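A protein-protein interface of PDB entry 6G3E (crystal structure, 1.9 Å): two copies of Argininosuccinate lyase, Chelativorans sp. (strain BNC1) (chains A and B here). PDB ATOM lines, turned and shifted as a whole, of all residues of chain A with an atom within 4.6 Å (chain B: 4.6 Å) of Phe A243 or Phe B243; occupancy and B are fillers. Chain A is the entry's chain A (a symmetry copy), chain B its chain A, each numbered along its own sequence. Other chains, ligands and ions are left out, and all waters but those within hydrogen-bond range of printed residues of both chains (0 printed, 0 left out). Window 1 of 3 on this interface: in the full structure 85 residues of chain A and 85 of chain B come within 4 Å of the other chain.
The guanidinium group of Arg B185 lies within salt-bridge range of the side-chain carboxylate of Glu A240. The side-chain carboxylate of Glu B240 lies within salt-bridge range of the guanidinium group of Arg A185 (2.8 Å).
Ala A239 touches Phe B243. Glu A240 touches Phe B243 (CA to CZ, 3.4 Å). O of Ala B239 touches CE1 of Phe A243, at 3.6 Å. CZ of Phe A243 touches CA of Glu B240 (3.4 Å). Phe B243 touches Phe A243. Leu B310 touches Val A247. CD2 of Leu A306 touches CD1 of Leu B310 (3.6 Å). CD2 of Leu A310 touches CA of Val B247, at 3.9 Å. Leu A310 touches Leu B306.
Phe A243 touches just these residues of chain B: Ala B239 (3.6 Å), Glu B240 (3.4 Å) and Phe B243 (3.5 Å). Of the printed residues of chain A, Glu B240 touches Arg A185 (2.8 Å) and Phe A243 (3.4 Å). Of the printed residues of chain B, Arg A185 touches Glu B240 (2.8 Å). Of the printed residues of chain A, Val B247 touches Leu A310. Printed residues of chain A within 4 Å of Ala B239: Phe A243. Printed residues of chain B within 4 Å of Glu A240: Arg B185 (2.8 Å) and Phe B243 (3.4 Å). Val B244 touches none of the printed residues of chain A. Asn A245 touches none of the printed residues of chain B. The nearest residue of chain B that does not touch Phe A243 is Leu B306 (4.1 Å). The nearest printed residue of chain B that does not touch Glu A240 is Val B247 (5.4 Å).
Of the 12 printed residues of chain B, 7 touch a printed residue of chain A. Printed residues of chain B that touch a printed residue of chain A: Arg B185, Ala B239, Glu B240, Phe B243, Val B247, Leu B306 and Leu B310. Among the printed residues, 11 pairs touch across the chains. Among the printed residues, Asp or Glu carboxylates within 4 Å of a Lys or Arg side-chain nitrogen of the other chain: Arg A185 with Glu B240 (2.8 Å) and Glu A240 with Arg B185 (2.8 Å).
Ala A239 touches Phe B243, and with the chains exchanged Phe A243 touches Ala B239. Glu A240 touches Phe B243, and with the chains exchanged Phe A243 touches Glu B240. Phe B243 touches its own counterpart, Phe A243. Leu A306 touches Leu B310, and with the chains exchanged Leu A310 touches Leu B306.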
ATOM      1  N   ARG A 185       9.529  34.105   2.438  1.00  0.00           N
ATOM      2  CA  ARG A 185       9.810  32.767   2.969  1.00  0.00           C
ATOM      3  C   ARG A 185       8.703  31.810   2.593  1.00  0.00           C
ATOM      4  O   ARG A 185       8.961  30.699   2.139  1.00  0.00           O
ATOM      5  CB  ARG A 185       9.970  32.778   4.492  1.00  0.00           C
ATOM      6  CG  ARG A 185      11.292  33.344   4.960  1.00  0.00           C
ATOM      7  CD  ARG A 185      11.512  33.200   6.474  1.00  0.00           C
ATOM      8  NE  ARG A 185      12.785  33.821   6.816  1.00  0.00           N
ATOM      9  CZ  ARG A 185      12.932  35.070   7.254  1.00  0.00           C
ATOM     10  NH1 ARG A 185      11.878  35.840   7.502  1.00  0.00           N
ATOM     11  NH2 ARG A 185      14.150  35.538   7.475  1.00  0.00           N
ATOM     12  N   ALA A 239       9.243  20.263   7.535  1.00  0.00           N
ATOM     13  CA  ALA A 239      10.106  20.957   8.482  1.00  0.00           C
ATOM     14  C   ALA A 239      10.170  22.452   8.163  1.00  0.00           C
ATOM     15  O   ALA A 239      10.139  23.292   9.066  1.00  0.00           O
ATOM     16  CB  ALA A 239      11.499  20.351   8.467  1.00  0.00           C
ATOM     17  N   GLU A 240      10.251  22.782   6.877  1.00  0.00           N
ATOM     18  CA  GLU A 240      10.379  24.172   6.464  1.00  0.00           C
ATOM     19  C   GLU A 240       9.083  24.920   6.746  1.00  0.00           C
ATOM     20  O   GLU A 240       9.109  26.070   7.196  1.00  0.00           O
ATOM     21  CB  GLU A 240      10.748  24.277   4.981  1.00  0.00           C
ATOM     22  CG  GLU A 240      11.024  25.703   4.526  1.00  0.00           C
ATOM     23  CD  GLU A 240      11.419  25.802   3.062  1.00  0.00           C
ATOM     24  OE1 GLU A 240      11.690  24.757   2.425  1.00  0.00           O
ATOM     25  OE2 GLU A 240      11.454  26.941   2.552  1.00  0.00           O
ATOM     26  N   HIS A 241       7.953  24.269   6.494  1.00  0.00           N
ATOM     27  CA  HIS A 241       6.658  24.870   6.797  1.00  0.00           C
ATOM     28  C   HIS A 241       6.573  25.177   8.285  1.00  0.00           C
ATOM     29  O   HIS A 241       6.178  26.277   8.679  1.00  0.00           O
ATOM     30  CB  HIS A 241       5.520  23.943   6.362  1.00  0.00           C
ATOM     31  CG  HIS A 241       4.178  24.607   6.321  1.00  0.00           C
ATOM     32  ND1 HIS A 241       3.138  24.132   5.550  1.00  0.00           N
ATOM     33  CD2 HIS A 241       3.708  25.713   6.946  1.00  0.00           C
ATOM     34  CE1 HIS A 241       2.084  24.912   5.709  1.00  0.00           C
ATOM     35  NE2 HIS A 241       2.404  25.880   6.551  1.00  0.00           N
ATOM     36  N   ALA A 242       6.970  24.220   9.116  1.00  0.00           N
ATOM     37  CA  ALA A 242       6.955  24.440  10.559  1.00  0.00           C
ATOM     38  C   ALA A 242       7.918  25.556  10.954  1.00  0.00           C
ATOM     39  O   ALA A 242       7.629  26.333  11.869  1.00  0.00           O
ATOM     40  CB  ALA A 242       7.296  23.156  11.303  1.00  0.00           C
ATOM     41  N   PHE A 243       9.055  25.653  10.269  1.00  0.00           N
ATOM     42  CA  PHE A 243      10.000  26.714  10.594  1.00  0.00           C
ATOM     43  C   PHE A 243       9.478  28.110  10.256  1.00  0.00           C
ATOM     44  O   PHE A 243       9.575  29.021  11.077  1.00  0.00           O
ATOM     45  CB  PHE A 243      11.338  26.559   9.882  1.00  0.00           C
ATOM     46  CG  PHE A 243      12.170  27.801   9.981  1.00  0.00           C
ATOM     47  CD1 PHE A 243      12.745  28.153  11.188  1.00  0.00           C
ATOM     48  CD2 PHE A 243      12.315  28.655   8.896  1.00  0.00           C
ATOM     49  CE1 PHE A 243      13.470  29.325  11.314  1.00  0.00           C
ATOM     50  CE2 PHE A 243      13.054  29.818   9.012  1.00  0.00           C
ATOM     51  CZ  PHE A 243      13.629  30.152  10.220  1.00  0.00           C
ATOM     52  N   VAL A 244       8.974  28.303   9.039  1.00  0.00           N
ATOM     53  CA  VAL A 244       8.510  29.628   8.657  1.00  0.00           C
ATOM     54  C   VAL A 244       7.377  30.042   9.594  1.00  0.00           C
ATOM     55  O   VAL A 244       7.311  31.199  10.009  1.00  0.00           O
ATOM     56  CB  VAL A 244       8.042  29.696   7.189  1.00  0.00           C
ATOM     57  CG1 VAL A 244       7.613  31.119   6.844  1.00  0.00           C
ATOM     58  CG2 VAL A 244       9.152  29.261   6.252  1.00  0.00           C
ATOM     59  N   ASN A 245       6.510  29.098   9.961  1.00  0.00           N
ATOM     60  CA  ASN A 245       5.483  29.376  10.965  1.00  0.00           C
ATOM     61  C   ASN A 245       6.103  29.896  12.262  1.00  0.00           C
ATOM     62  O   ASN A 245       5.663  30.907  12.816  1.00  0.00           O
ATOM     63  CB  ASN A 245       4.654  28.122  11.265  1.00  0.00           C
ATOM     64  CG  ASN A 245       3.635  27.817  10.188  1.00  0.00           C
ATOM     65  OD1 ASN A 245       3.563  28.502   9.164  1.00  0.00           O
ATOM     66  ND2 ASN A 245       2.837  26.775  10.412  1.00  0.00           N
ATOM     67  N   ALA A 246       7.135  29.205  12.738  1.00  0.00           N
ATOM     68  CA  ALA A 246       7.767  29.556  14.003  1.00  0.00           C
ATOM     69  C   ALA A 246       8.459  30.920  13.950  1.00  0.00           C
ATOM     70  O   ALA A 246       8.314  31.726  14.868  1.00  0.00           O
ATOM     71  CB  ALA A 246       8.758  28.485  14.410  1.00  0.00           C
ATOM     72  N   VAL A 247       9.214  31.192  12.889  1.00  0.00           N
ATOM     73  CA  VAL A 247       9.943  32.453  12.832  1.00  0.00           C
ATOM     74  C   VAL A 247       8.979  33.610  12.583  1.00  0.00           C
ATOM     75  O   VAL A 247       9.142  34.677  13.178  1.00  0.00           O
ATOM     76  CB  VAL A 247      11.065  32.448  11.766  1.00  0.00           C
ATOM     77  CG1 VAL A 247      10.514  32.542  10.346  1.00  0.00           C
ATOM     78  CG2 VAL A 247      12.040  33.592  12.046  1.00  0.00           C
ATOM     79  N   LEU A 306       8.101  22.135  15.016  1.00  0.00           N
ATOM     80  CA  LEU A 306       9.389  22.299  14.367  1.00  0.00           C
ATOM     81  C   LEU A 306      10.424  21.341  14.947  1.00  0.00           C
ATOM     82  O   LEU A 306      11.140  20.662  14.211  1.00  0.00           O
ATOM     83  CB  LEU A 306       9.864  23.746  14.505  1.00  0.00           C
ATOM     84  CG  LEU A 306      11.281  24.046  14.015  1.00  0.00           C
ATOM     85  CD1 LEU A 306      11.420  23.695  12.540  1.00  0.00           C
ATOM     86  CD2 LEU A 306      11.620  25.505  14.259  1.00  0.00           C
ATOM     87  N   LEU A 310      11.960  17.868  13.018  1.00  0.00           N
ATOM     88  CA  LEU A 310      13.396  17.750  12.773  1.00  0.00           C
ATOM     89  C   LEU A 310      14.014  16.605  13.563  1.00  0.00           C
ATOM     90  O   LEU A 310      14.926  15.932  13.081  1.00  0.00           O
ATOM     91  CB  LEU A 310      14.112  19.052  13.114  1.00  0.00           C
ATOM     92  CG  LEU A 310      13.934  20.165  12.080  1.00  0.00           C
ATOM     93  CD1 LEU A 310      14.412  21.495  12.629  1.00  0.00           C
ATOM     94  CD2 LEU A 310      14.687  19.822  10.803  1.00  0.00           C
ATOM     95  N   ARG B 185      17.407  26.668  -0.663  1.00  0.00           N
ATOM     96  CA  ARG B 185      17.151  27.263   0.653  1.00  0.00           C
ATOM     97  C   ARG B 185      18.259  28.225   1.019  1.00  0.00           C
ATOM     98  O   ARG B 185      18.000  29.338   1.467  1.00  0.00           O
ATOM     99  CB  ARG B 185      17.027  26.199   1.748  1.00  0.00           C
ATOM    100  CG  ARG B 185      15.711  25.454   1.724  1.00  0.00           C
ATOM    101  CD  ARG B 185      15.528  24.507   2.921  1.00  0.00           C
ATOM    102  NE  ARG B 185      14.258  23.810   2.767  1.00  0.00           N
ATOM    103  CZ  ARG B 185      14.109  22.604   2.222  1.00  0.00           C
ATOM    104  NH1 ARG B 185      15.161  21.887   1.842  1.00  0.00           N
ATOM    105  NH2 ARG B 185      12.892  22.103   2.085  1.00  0.00           N
ATOM    106  N   ALA B 239      17.944  33.125  12.592  1.00  0.00           N
ATOM    107  CA  ALA B 239      17.097  31.960  12.814  1.00  0.00           C
ATOM    108  C   ALA B 239      17.012  31.102  11.550  1.00  0.00           C
ATOM    109  O   ALA B 239      17.056  29.872  11.619  1.00  0.00           O
ATOM    110  CB  ALA B 239      15.710  32.394  13.256  1.00  0.00           C
ATOM    111  N   GLU B 240      16.897  31.754  10.397  1.00  0.00           N
ATOM    112  CA  GLU B 240      16.747  31.036   9.139  1.00  0.00           C
ATOM    113  C   GLU B 240      18.041  30.314   8.794  1.00  0.00           C
ATOM    114  O   GLU B 240      18.015  29.173   8.323  1.00  0.00           O
ATOM    115  CB  GLU B 240      16.342  31.984   8.006  1.00  0.00           C
ATOM    116  CG  GLU B 240      16.042  31.268   6.697  1.00  0.00           C
ATOM    117  CD  GLU B 240      15.611  32.207   5.583  1.00  0.00           C
ATOM    118  OE1 GLU B 240      15.335  33.399   5.854  1.00  0.00           O
ATOM    119  OE2 GLU B 240      15.553  31.739   4.427  1.00  0.00           O
ATOM    120  N   HIS B 241      19.171  30.968   9.037  1.00  0.00           N
ATOM    121  CA  HIS B 241      20.467  30.338   8.809  1.00  0.00           C
ATOM    122  C   HIS B 241      20.584  29.086   9.666  1.00  0.00           C
ATOM    123  O   HIS B 241      20.979  28.024   9.179  1.00  0.00           O
ATOM    124  CB  HIS B 241      21.603  31.318   9.110  1.00  0.00           C
ATOM    125  CG  HIS B 241      22.938  30.881   8.589  1.00  0.00           C
ATOM    126  ND1 HIS B 241      23.964  31.767   8.338  1.00  0.00           N
ATOM    127  CD2 HIS B 241      23.412  29.654   8.262  1.00  0.00           C
ATOM    128  CE1 HIS B 241      25.014  31.104   7.887  1.00  0.00           C
ATOM    129  NE2 HIS B 241      24.705  29.819   7.832  1.00  0.00           N
ATOM    130  N   ALA B 242      20.216  29.197  10.938  1.00  0.00           N
ATOM    131  CA  ALA B 242      20.263  28.039  11.825  1.00  0.00           C
ATOM    132  C   ALA B 242      19.299  26.951  11.360  1.00  0.00           C
ATOM    133  O   ALA B 242      19.603  25.760  11.475  1.00  0.00           O
ATOM    134  CB  ALA B 242      19.952  28.447  13.259  1.00  0.00           C
ATOM    135  N   PHE B 243      18.145  27.345  10.826  1.00  0.00           N
ATOM    136  CA  PHE B 243      17.198  26.346  10.347  1.00  0.00           C
ATOM    137  C   PHE B 243      17.699  25.578   9.125  1.00  0.00           C
ATOM    138  O   PHE B 243      17.613  24.351   9.088  1.00  0.00           O
ATOM    139  CB  PHE B 243      15.845  26.938   9.974  1.00  0.00           C
ATOM    140  CG  PHE B 243      15.004  25.966   9.204  1.00  0.00           C
ATOM    141  CD1 PHE B 243      14.455  24.871   9.844  1.00  0.00           C
ATOM    142  CD2 PHE B 243      14.825  26.100   7.834  1.00  0.00           C
ATOM    143  CE1 PHE B 243      13.722  23.932   9.140  1.00  0.00           C
ATOM    144  CE2 PHE B 243      14.078  25.174   7.129  1.00  0.00           C
ATOM    145  CZ  PHE B 243      13.529  24.091   7.782  1.00  0.00           C
ATOM    146  N   VAL B 244      18.172  26.287   8.102  1.00  0.00           N
ATOM    147  CA  VAL B 244      18.615  25.600   6.898  1.00  0.00           C
ATOM    148  C   VAL B 244      19.765  24.663   7.260  1.00  0.00           C
ATOM    149  O   VAL B 244      19.830  23.541   6.756  1.00  0.00           O
ATOM    150  CB  VAL B 244      19.047  26.572   5.781  1.00  0.00           C
ATOM    151  CG1 VAL B 244      19.454  25.789   4.537  1.00  0.00           C
ATOM    152  CG2 VAL B 244      17.920  27.524   5.433  1.00  0.00           C
ATOM    153  N   ASN B 245      20.650  25.098   8.157  1.00  0.00           N
ATOM    154  CA  ASN B 245      21.697  24.212   8.665  1.00  0.00           C
ATOM    155  C   ASN B 245      21.103  22.932   9.254  1.00  0.00           C
ATOM    156  O   ASN B 245      21.547  21.824   8.943  1.00  0.00           O
ATOM    157  CB  ASN B 245      22.545  24.916   9.730  1.00  0.00           C
ATOM    158  CG  ASN B 245      23.541  25.892   9.141  1.00  0.00           C
ATOM    159  OD1 ASN B 245      23.583  26.108   7.926  1.00  0.00           O
ATOM    160  ND2 ASN B 245      24.354  26.496  10.006  1.00  0.00           N
ATOM    161  N   ALA B 246      20.089  23.092  10.100  1.00  0.00           N
ATOM    162  CA  ALA B 246      19.484  21.956  10.784  1.00  0.00           C
ATOM    163  C   ALA B 246      18.778  21.003   9.817  1.00  0.00           C
ATOM    164  O   ALA B 246      18.937  19.787   9.918  1.00  0.00           O
ATOM    165  CB  ALA B 246      18.513  22.438  11.843  1.00  0.00           C
ATOM    166  N   VAL B 247      17.996  21.534   8.882  1.00  0.00           N
ATOM    167  CA  VAL B 247      17.254  20.657   7.985  1.00  0.00           C
ATOM    168  C   VAL B 247      18.201  20.004   6.981  1.00  0.00           C
ATOM    169  O   VAL B 247      18.041  18.821   6.674  1.00  0.00           O
ATOM    170  CB  VAL B 247      16.107  21.389   7.246  1.00  0.00           C
ATOM    171  CG1 VAL B 247      16.624  22.309   6.144  1.00  0.00           C
ATOM    172  CG2 VAL B 247      15.128  20.360   6.678  1.00  0.00           C
ATOM    173  N   LEU B 306      19.244  26.604  16.662  1.00  0.00           N
ATOM    174  CA  LEU B 306      17.940  26.923  16.110  1.00  0.00           C
ATOM    175  C   LEU B 306      16.928  27.203  17.217  1.00  0.00           C
ATOM    176  O   LEU B 306      16.202  28.196  17.174  1.00  0.00           O
ATOM    177  CB  LEU B 306      17.454  25.780  15.219  1.00  0.00           C
ATOM    178  CG  LEU B 306      16.024  25.889  14.692  1.00  0.00           C
ATOM    179  CD1 LEU B 306      15.853  27.163  13.875  1.00  0.00           C
ATOM    180  CD2 LEU B 306      15.676  24.665  13.866  1.00  0.00           C
ATOM    181  N   LEU B 310      15.380  31.029  18.268  1.00  0.00           N
ATOM    182  CA  LEU B 310      13.939  31.270  18.207  1.00  0.00           C
ATOM    183  C   LEU B 310      13.351  31.543  19.584  1.00  0.00           C
ATOM    184  O   LEU B 310      12.434  32.354  19.724  1.00  0.00           O
ATOM    185  CB  LEU B 310      13.219  30.088  17.567  1.00  0.00           C
ATOM    186  CG  LEU B 310      13.363  30.003  16.047  1.00  0.00           C
ATOM    187  CD1 LEU B 310      12.885  28.660  15.533  1.00  0.00           C
ATOM    188  CD2 LEU B 310      12.583  31.128  15.382  1.00  0.00           C
